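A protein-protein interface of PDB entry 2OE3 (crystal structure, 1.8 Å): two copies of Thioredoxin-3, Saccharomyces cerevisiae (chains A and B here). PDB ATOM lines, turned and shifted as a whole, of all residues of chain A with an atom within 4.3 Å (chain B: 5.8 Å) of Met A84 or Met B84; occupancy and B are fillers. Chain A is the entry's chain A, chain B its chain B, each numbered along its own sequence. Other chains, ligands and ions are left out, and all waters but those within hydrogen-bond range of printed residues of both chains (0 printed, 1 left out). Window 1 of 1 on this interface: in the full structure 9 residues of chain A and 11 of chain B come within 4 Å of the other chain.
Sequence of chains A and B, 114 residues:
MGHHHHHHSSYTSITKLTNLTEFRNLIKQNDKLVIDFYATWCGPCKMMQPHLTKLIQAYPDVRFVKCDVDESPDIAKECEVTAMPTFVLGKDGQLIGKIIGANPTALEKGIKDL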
ATOM      1  N   PHE A  37       2.484  -3.748  14.776  1.00  0.00           N
ATOM      2  CA  PHE A  37       3.515  -3.537  15.790  1.00  0.00           C
ATOM      3  C   PHE A  37       2.894  -2.816  16.980  1.00  0.00           C
ATOM      4  O   PHE A  37       2.479  -1.645  16.872  1.00  0.00           O
ATOM      5  CB  PHE A  37       4.723  -2.756  15.259  1.00  0.00           C
ATOM      6  CG  PHE A  37       5.623  -3.564  14.362  1.00  0.00           C
ATOM      7  CD1 PHE A  37       5.448  -3.533  12.988  1.00  0.00           C
ATOM      8  CD2 PHE A  37       6.627  -4.383  14.899  1.00  0.00           C
ATOM      9  CE1 PHE A  37       6.295  -4.301  12.137  1.00  0.00           C
ATOM     10  CE2 PHE A  37       7.472  -5.151  14.074  1.00  0.00           C
ATOM     11  CZ  PHE A  37       7.296  -5.113  12.684  1.00  0.00           C
ATOM     12  N   TYR A  38       2.825  -3.533  18.098  1.00  0.00           N
ATOM     13  CA  TYR A  38       2.174  -3.042  19.312  1.00  0.00           C
ATOM     14  C   TYR A  38       3.070  -3.238  20.526  1.00  0.00           C
ATOM     15  O   TYR A  38       4.131  -3.850  20.432  1.00  0.00           O
ATOM     16  CB  TYR A  38       0.831  -3.753  19.508  1.00  0.00           C
ATOM     17  CG  TYR A  38       0.981  -5.170  19.979  1.00  0.00           C
ATOM     18  CD1 TYR A  38       0.791  -5.508  21.335  1.00  0.00           C
ATOM     19  CD2 TYR A  38       1.306  -6.185  19.078  1.00  0.00           C
ATOM     20  CE1 TYR A  38       0.927  -6.843  21.770  1.00  0.00           C
ATOM     21  CE2 TYR A  38       1.457  -7.505  19.498  1.00  0.00           C
ATOM     22  CZ  TYR A  38       1.257  -7.830  20.834  1.00  0.00           C
ATOM     23  OH  TYR A  38       1.419  -9.140  21.232  1.00  0.00           O
ATOM     24  N   ALA A  39       2.649  -2.642  21.643  1.00  0.00           N
ATOM     25  CA  ALA A  39       3.242  -2.898  22.943  1.00  0.00           C
ATOM     26  C   ALA A  39       2.113  -3.056  23.952  1.00  0.00           C
ATOM     27  O   ALA A  39       1.067  -2.428  23.823  1.00  0.00           O
ATOM     28  CB  ALA A  39       4.130  -1.740  23.354  1.00  0.00           C
ATOM     29  N   TRP A  41       1.893  -1.857  26.998  1.00  0.00           N
ATOM     30  CA  TRP A  41       1.639  -0.558  27.648  1.00  0.00           C
ATOM     31  C   TRP A  41       0.942   0.469  26.753  1.00  0.00           C
ATOM     32  O   TRP A  41       0.642   1.577  27.193  1.00  0.00           O
ATOM     33  CB  TRP A  41       2.952   0.054  28.157  1.00  0.00           C
ATOM     34  CG  TRP A  41       4.105  -0.107  27.200  1.00  0.00           C
ATOM     35  CD1 TRP A  41       5.084  -1.063  27.243  1.00  0.00           C
ATOM     36  CD2 TRP A  41       4.374   0.693  26.043  1.00  0.00           C
ATOM     37  NE1 TRP A  41       5.954  -0.901  26.192  1.00  0.00           N
ATOM     38  CE2 TRP A  41       5.549   0.174  25.443  1.00  0.00           C
ATOM     39  CE3 TRP A  41       3.723   1.797  25.444  1.00  0.00           C
ATOM     40  CZ2 TRP A  41       6.099   0.712  24.265  1.00  0.00           C
ATOM     41  CZ3 TRP A  41       4.280   2.344  24.265  1.00  0.00           C
ATOM     42  CH2 TRP A  41       5.458   1.786  23.690  1.00  0.00           C
ATOM     43  N   CYS A  42       0.668   0.101  25.509  1.00  0.00           N
ATOM     44  CA  CYS A  42       0.187   1.075  24.522  1.00  0.00           C
ATOM     45  C   CYS A  42      -1.340   1.136  24.406  1.00  0.00           C
ATOM     46  O   CYS A  42      -1.975   0.234  23.862  1.00  0.00           O
ATOM     47  CB  CYS A  42       0.809   0.759  23.150  1.00  0.00           C
ATOM     48  SG  CYS A  42       0.219   1.743  21.759  1.00  0.00           S
ATOM     49  N   PRO A  44      -3.520   3.356  22.741  1.00  0.00           N
ATOM     50  CA  PRO A  44      -4.074   3.503  21.385  1.00  0.00           C
ATOM     51  C   PRO A  44      -3.950   2.193  20.593  1.00  0.00           C
ATOM     52  O   PRO A  44      -4.807   1.906  19.740  1.00  0.00           O
ATOM     53  CB  PRO A  44      -3.218   4.604  20.783  1.00  0.00           C
ATOM     54  CG  PRO A  44      -2.772   5.424  22.022  1.00  0.00           C
ATOM     55  CD  PRO A  44      -2.420   4.307  22.982  1.00  0.00           C
ATOM     56  N   CYS A  45      -2.925   1.385  20.901  1.00  0.00           N
ATOM     57  CA  CYS A  45      -2.804   0.069  20.293  1.00  0.00           C
ATOM     58  C   CYS A  45      -3.998  -0.819  20.664  1.00  0.00           C
ATOM     59  O   CYS A  45      -4.567  -1.524  19.823  1.00  0.00           O
ATOM     60  CB  CYS A  45      -1.507  -0.621  20.746  1.00  0.00           C
ATOM     61  SG  CYS A  45       0.026   0.243  20.302  1.00  0.00           S
ATOM     62  N   VAL A  69       6.730  -5.312  20.236  1.00  0.00           N
ATOM     63  CA  VAL A  69       8.028  -4.663  20.054  1.00  0.00           C
ATOM     64  C   VAL A  69       9.009  -4.880  21.220  1.00  0.00           C
ATOM     65  O   VAL A  69      10.224  -4.814  21.033  1.00  0.00           O
ATOM     66  CB  VAL A  69       7.897  -3.135  19.731  1.00  0.00           C
ATOM     67  CG1 VAL A  69       7.117  -2.913  18.412  1.00  0.00           C
ATOM     68  CG2 VAL A  69       7.275  -2.356  20.905  1.00  0.00           C
ATOM     69  N   VAL A  81      10.635   0.762  13.614  1.00  0.00           N
ATOM     70  CA  VAL A  81       9.385   1.098  14.306  1.00  0.00           C
ATOM     71  C   VAL A  81       9.749   2.072  15.431  1.00  0.00           C
ATOM     72  O   VAL A  81      10.395   1.670  16.406  1.00  0.00           O
ATOM     73  CB  VAL A  81       8.696  -0.180  14.867  1.00  0.00           C
ATOM     74  CG1 VAL A  81       7.402   0.198  15.659  1.00  0.00           C
ATOM     75  CG2 VAL A  81       8.374  -1.100  13.713  1.00  0.00           C
ATOM     76  N   THR A  82       9.384   3.345  15.287  1.00  0.00           N
ATOM     77  CA  THR A  82       9.790   4.378  16.252  1.00  0.00           C
ATOM     78  C   THR A  82       8.577   5.024  16.940  1.00  0.00           C
ATOM     79  O   THR A  82       8.725   5.898  17.787  1.00  0.00           O
ATOM     80  CB  THR A  82      10.665   5.491  15.580  1.00  0.00           C
ATOM     81  OG1 THR A  82       9.869   6.164  14.608  1.00  0.00           O
ATOM     82  CG2 THR A  82      11.916   4.861  14.855  1.00  0.00           C
ATOM     83  N   ALA A  83       7.379   4.592  16.564  1.00  0.00           N
ATOM     84  CA  ALA A  83       6.138   5.113  17.165  1.00  0.00           C
ATOM     85  C   ALA A  83       5.129   3.993  17.284  1.00  0.00           C
ATOM     86  O   ALA A  83       5.042   3.165  16.385  1.00  0.00           O
ATOM     87  CB  ALA A  83       5.540   6.187  16.296  1.00  0.00           C
ATOM     88  N   MET A  84       4.316   4.026  18.333  1.00  0.00           N
ATOM     89  CA  MET A  84       3.337   2.967  18.548  1.00  0.00           C
ATOM     90  C   MET A  84       1.917   3.526  18.448  1.00  0.00           C
ATOM     91  O   MET A  84       1.649   4.616  18.975  1.00  0.00           O
ATOM     92  CB  MET A  84       3.558   2.325  19.918  1.00  0.00           C
ATOM     93  CG  MET A  84       4.984   1.811  20.126  1.00  0.00           C
ATOM     94  SD  MET A  84       5.430   0.608  18.856  1.00  0.00           S
ATOM     95  CE  MET A  84       4.349  -0.655  19.361  1.00  0.00           C
ATOM     96  N   PRO A  85       1.000   2.793  17.781  1.00  0.00           N
ATOM     97  CA  PRO A  85       1.214   1.569  17.006  1.00  0.00           C
ATOM     98  C   PRO A  85       1.839   1.939  15.651  1.00  0.00           C
ATOM     99  O   PRO A  85       1.754   3.119  15.247  1.00  0.00           O
ATOM    100  CB  PRO A  85      -0.215   1.050  16.777  1.00  0.00           C
ATOM    101  CG  PRO A  85      -1.053   2.286  16.690  1.00  0.00           C
ATOM    102  CD  PRO A  85      -0.421   3.201  17.773  1.00  0.00           C
ATOM    103  N   THR A  86       2.416   0.935  14.983  1.00  0.00           N
ATOM    104  CA  THR A  86       2.794   1.010  13.588  1.00  0.00           C
ATOM    105  C   THR A  86       2.322  -0.226  12.864  1.00  0.00           C
ATOM    106  O   THR A  86       2.518  -1.357  13.336  1.00  0.00           O
ATOM    107  CB  THR A  86       4.323   1.120  13.372  1.00  0.00           C
ATOM    108  OG1 THR A  86       4.770   2.404  13.803  1.00  0.00           O
ATOM    109  CG2 THR A  86       4.674   0.954  11.879  1.00  0.00           C
ATOM    110  N   PHE B  37       4.336  14.320  23.664  1.00  0.00           N
ATOM    111  CA  PHE B  37       3.211  13.473  23.980  1.00  0.00           C
ATOM    112  C   PHE B  37       3.745  12.053  24.137  1.00  0.00           C
ATOM    113  O   PHE B  37       4.229  11.453  23.181  1.00  0.00           O
ATOM    114  CB  PHE B  37       2.151  13.556  22.866  1.00  0.00           C
ATOM    115  CG  PHE B  37       1.300  14.804  22.913  1.00  0.00           C
ATOM    116  CD1 PHE B  37       0.154  14.853  23.719  1.00  0.00           C
ATOM    117  CD2 PHE B  37       1.600  15.908  22.130  1.00  0.00           C
ATOM    118  CE1 PHE B  37      -0.662  15.996  23.762  1.00  0.00           C
ATOM    119  CE2 PHE B  37       0.780  17.058  22.155  1.00  0.00           C
ATOM    120  CZ  PHE B  37      -0.350  17.112  22.964  1.00  0.00           C
ATOM    121  N   TYR B  38       3.619  11.517  25.346  1.00  0.00           N
ATOM    122  CA  TYR B  38       4.199  10.225  25.700  1.00  0.00           C
ATOM    123  C   TYR B  38       3.179   9.424  26.482  1.00  0.00           C
ATOM    124  O   TYR B  38       2.097   9.926  26.763  1.00  0.00           O
ATOM    125  CB  TYR B  38       5.443  10.445  26.555  1.00  0.00           C
ATOM    126  CG  TYR B  38       5.122  10.965  27.945  1.00  0.00           C
ATOM    127  CD1 TYR B  38       5.104  10.112  29.054  1.00  0.00           C
ATOM    128  CD2 TYR B  38       4.861  12.317  28.152  1.00  0.00           C
ATOM    129  CE1 TYR B  38       4.814  10.603  30.326  1.00  0.00           C
ATOM    130  CE2 TYR B  38       4.574  12.817  29.436  1.00  0.00           C
ATOM    131  CZ  TYR B  38       4.544  11.943  30.504  1.00  0.00           C
ATOM    132  OH  TYR B  38       4.265  12.439  31.751  1.00  0.00           O
ATOM    133  N   ALA B  39       3.550   8.192  26.841  1.00  0.00           N
ATOM    134  CA  ALA B  39       2.838   7.381  27.823  1.00  0.00           C
ATOM    135  C   ALA B  39       3.857   6.792  28.767  1.00  0.00           C
ATOM    136  O   ALA B  39       5.021   6.576  28.416  1.00  0.00           O
ATOM    137  CB  ALA B  39       2.071   6.232  27.155  1.00  0.00           C
ATOM    138  N   CYS B  42       6.410   3.626  27.925  1.00  0.00           N
ATOM    139  CA  CYS B  42       6.682   3.631  26.491  1.00  0.00           C
ATOM    140  C   CYS B  42       8.188   3.670  26.179  1.00  0.00           C
ATOM    141  O   CYS B  42       8.884   4.624  26.539  1.00  0.00           O
ATOM    142  CB  CYS B  42       5.991   4.845  25.886  1.00  0.00           C
ATOM    143  SG  CYS B  42       6.471   5.270  24.229  1.00  0.00           S
ATOM    144  N   PRO B  44      10.111   3.763  23.135  1.00  0.00           N
ATOM    145  CA  PRO B  44      10.634   4.850  22.279  1.00  0.00           C
ATOM    146  C   PRO B  44      10.572   6.208  22.986  1.00  0.00           C
ATOM    147  O   PRO B  44      11.473   7.012  22.838  1.00  0.00           O
ATOM    148  CB  PRO B  44       9.688   4.840  21.072  1.00  0.00           C
ATOM    149  CG  PRO B  44       9.102   3.410  21.054  1.00  0.00           C
ATOM    150  CD  PRO B  44       8.983   3.044  22.506  1.00  0.00           C
ATOM    151  N   CYS B  45       9.504   6.442  23.747  1.00  0.00           N
ATOM    152  CA  CYS B  45       9.337   7.694  24.536  1.00  0.00           C
ATOM    153  C   CYS B  45      10.537   7.888  25.474  1.00  0.00           C
ATOM    154  O   CYS B  45      11.199   8.941  25.467  1.00  0.00           O
ATOM    155  CB  CYS B  45       8.034   7.636  25.354  1.00  0.00           C
ATOM    156  SG  CYS B  45       6.533   7.335  24.372  1.00  0.00           S
ATOM    157  N   VAL B  69      -0.530  11.027  27.298  1.00  0.00           N
ATOM    158  CA  VAL B  69      -1.711  10.821  26.427  1.00  0.00           C
ATOM    159  C   VAL B  69      -2.856  10.039  27.103  1.00  0.00           C
ATOM    160  O   VAL B  69      -4.025  10.238  26.785  1.00  0.00           O
ATOM    161  CB  VAL B  69      -1.372  10.107  25.096  1.00  0.00           C
ATOM    162  CG1 VAL B  69      -0.419  10.963  24.217  1.00  0.00           C
ATOM    163  CG2 VAL B  69      -0.780   8.744  25.358  1.00  0.00           C
ATOM    164  N   ASP B  70      -2.504   9.134  28.009  1.00  0.00           N
ATOM    165  CA  ASP B  70      -3.506   8.393  28.785  1.00  0.00           C
ATOM    166  C   ASP B  70      -4.142   9.202  29.903  1.00  0.00           C
ATOM    167  O   ASP B  70      -5.316   9.006  30.201  1.00  0.00           O
ATOM    168  CB  ASP B  70      -2.904   7.129  29.382  1.00  0.00           C
ATOM    169  CG  ASP B  70      -2.476   6.161  28.335  1.00  0.00           C
ATOM    170  OD1 ASP B  70      -3.221   5.960  27.344  1.00  0.00           O
ATOM    171  OD2 ASP B  70      -1.371   5.614  28.494  1.00  0.00           O
ATOM    172  N   VAL B  81      -3.205  13.679  18.142  1.00  0.00           N
ATOM    173  CA  VAL B  81      -2.093  12.758  18.445  1.00  0.00           C
ATOM    174  C   VAL B  81      -2.633  11.339  18.458  1.00  0.00           C
ATOM    175  O   VAL B  81      -3.519  11.018  19.255  1.00  0.00           O
ATOM    176  CB  VAL B  81      -1.422  13.116  19.794  1.00  0.00           C
ATOM    177  CG1 VAL B  81      -0.424  11.991  20.242  1.00  0.00           C
ATOM    178  CG2 VAL B  81      -0.670  14.467  19.645  1.00  0.00           C
ATOM    179  N   THR B  82      -2.089  10.494  17.575  1.00  0.00           N
ATOM    180  CA  THR B  82      -2.551   9.111  17.487  1.00  0.00           C
ATOM    181  C   THR B  82      -1.469   8.043  17.666  1.00  0.00           C
ATOM    182  O   THR B  82      -1.752   6.838  17.592  1.00  0.00           O
ATOM    183  CB  THR B  82      -3.258   8.849  16.151  1.00  0.00           C
ATOM    184  OG1 THR B  82      -2.340   9.042  15.082  1.00  0.00           O
ATOM    185  CG2 THR B  82      -4.495   9.746  16.011  1.00  0.00           C
ATOM    186  N   ALA B  83      -0.243   8.483  17.919  1.00  0.00           N
ATOM    187  CA  ALA B  83       0.895   7.574  18.087  1.00  0.00           C
ATOM    188  C   ALA B  83       1.808   8.165  19.152  1.00  0.00           C
ATOM    189  O   ALA B  83       1.759   9.383  19.406  1.00  0.00           O
ATOM    190  CB  ALA B  83       1.649   7.456  16.750  1.00  0.00           C
ATOM    191  N   MET B  84       2.651   7.319  19.753  1.00  0.00           N
ATOM    192  CA  MET B  84       3.583   7.751  20.785  1.00  0.00           C
ATOM    193  C   MET B  84       4.999   7.239  20.495  1.00  0.00           C
ATOM    194  O   MET B  84       5.150   6.105  19.998  1.00  0.00           O
ATOM    195  CB  MET B  84       3.118   7.231  22.166  1.00  0.00           C
ATOM    196  CG  MET B  84       2.897   5.684  22.272  1.00  0.00           C
ATOM    197  SD  MET B  84       2.342   5.195  23.945  1.00  0.00           S
ATOM    198  CE  MET B  84       0.617   5.672  23.883  1.00  0.00           C
ATOM    199  N   PRO B  85       6.038   8.063  20.768  1.00  0.00           N
ATOM    200  CA  PRO B  85       5.885   9.474  21.178  1.00  0.00           C
ATOM    201  C   PRO B  85       5.513  10.357  19.950  1.00  0.00           C
ATOM    202  O   PRO B  85       5.856  10.005  18.806  1.00  0.00           O
ATOM    203  CB  PRO B  85       7.286   9.829  21.664  1.00  0.00           C
ATOM    204  CG  PRO B  85       8.197   9.040  20.724  1.00  0.00           C
ATOM    205  CD  PRO B  85       7.463   7.694  20.593  1.00  0.00           C
ATOM    206  N   THR B  86       4.783  11.451  20.172  1.00  0.00           N
ATOM    207  CA  THR B  86       4.663  12.505  19.149  1.00  0.00           C
ATOM    208  C   THR B  86       5.100  13.846  19.752  1.00  0.00           C
ATOM    209  O   THR B  86       4.682  14.219  20.857  1.00  0.00           O
ATOM    210  CB  THR B  86       3.195  12.639  18.667  1.00  0.00           C
ATOM    211  OG1 THR B  86       2.838  11.451  17.971  1.00  0.00           O
ATOM    212  CG2 THR B  86       3.014  13.868  17.715  1.00  0.00           C
ATOM    213  N   GLY B 101       7.114   9.855  16.336  1.00  0.00           N
ATOM    214  CA  GLY B 101       8.062   8.826  16.654  1.00  0.00           C
ATOM    215  C   GLY B 101       9.369   9.332  17.257  1.00  0.00           C
ATOM    216  O   GLY B 101       9.609  10.552  17.320  1.00  0.00           O
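The backbone NH of Met A84 sits at hydrogen-bond distance from the backbone carbonyl oxygen of Met B84, at 2.8 Å.
O of Ala A83 sits at hydrogen-bond distance from OG1 of Thr A86, 2.7 Å away.
SG of Cys B45 forms a disulfide with SG of Cys B42, 2.1 Å away.
O of Ala B83 is in hydrogen-bond range of OG1 of Thr B86.
The backbone carbonyl oxygen (O) of Pro B85 lies within hydrogen-bond range of the backbone NH (N) of Gly B101, 2.8 Å away.
The side-chain sulfur (SG) of Cys A45 is disulfide-bonded to the side-chain sulfur (SG) of Cys A42.
CB of Cys B42 touches CZ3 of Trp A41, 3.4 Å away.
Pro B44 touches Trp A41 (CD to CH2, 3.9 Å).
CZ3 of Trp A41 touches SD of Met B84 (3.5 Å).
Met B84 touches Pro A44.
O of Thr A82 touches CB of Pro B44 (3.6 Å).
O of Thr A82 touches CD of Pro B85, at 3.6 Å.
O of Thr A82 touches CA of Gly B101, at 3.2 Å.
Ala A83 touches Met B84.
Gly B101 touches Ala A83.
CA of Ala B83 touches O of Met A84, 3.2 Å away.
Of the printed residues of chain B, Trp A41 touches Cys B42 (3.4 Å), Pro B44 (3.9 Å) and Met B84 (3.5 Å).
Val A69 touches none of the printed residues of chain B.
Met A84 touches two residues of chain B.
Of the printed residues of chain B, Pro A85 touches Thr B82 (3.9 Å).
Of the printed residues of chain A, Cys B42 touches Trp A41.
Of chain A, only Trp A41 (3.5 Å), Pro A44 (3.4 Å), Ala A83 (3.2 Å) and Met A84 (2.8 Å) come within 4 Å of Met B84.
Of the printed residues of chain A, Pro B85 touches Thr A82.
Thr B86 touches none of the printed residues of chain A.
Printed residues of chain A within 4 Å of Gly B101: Thr A82 (3.2 Å) and Ala A83 (3.7 Å).
The nearest residue of chain B that does not touch Met A84 is Thr B82 (4.3 Å).
The nearest residue of chain A that does not touch Met B84 is Thr A82 (4.2 Å).
The nearest printed residue of chain A that does not touch Ala B83 is Ala A83 (4.1 Å).
Hydrophobic or aromatic side chains of chain B that line the printed part of chain A: Pro B44, Ala B83, Met B84 and Pro B85.
Among the printed residues, 12 pairs touch across the chains.
Among the printed residues, no Asp or Glu carboxylate lies within 4 Å of a Lys or Arg side-chain nitrogen of the other chain.
Pro A44 touches Met B84, but with the chains exchanged Met A84 does not touch Pro B44 (4.5 Å).
Thr A82 touches Pro B44, but with the chains exchanged Pro A44 does not touch Thr B82 (4.2 Å).
Thr A82 touches Pro B85, and with the chains exchanged Pro A85 touches Thr B82.
Ala A83 touches Met B84, and with the chains exchanged Met A84 touches Ala B83.
13 positions are printed for both chains.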
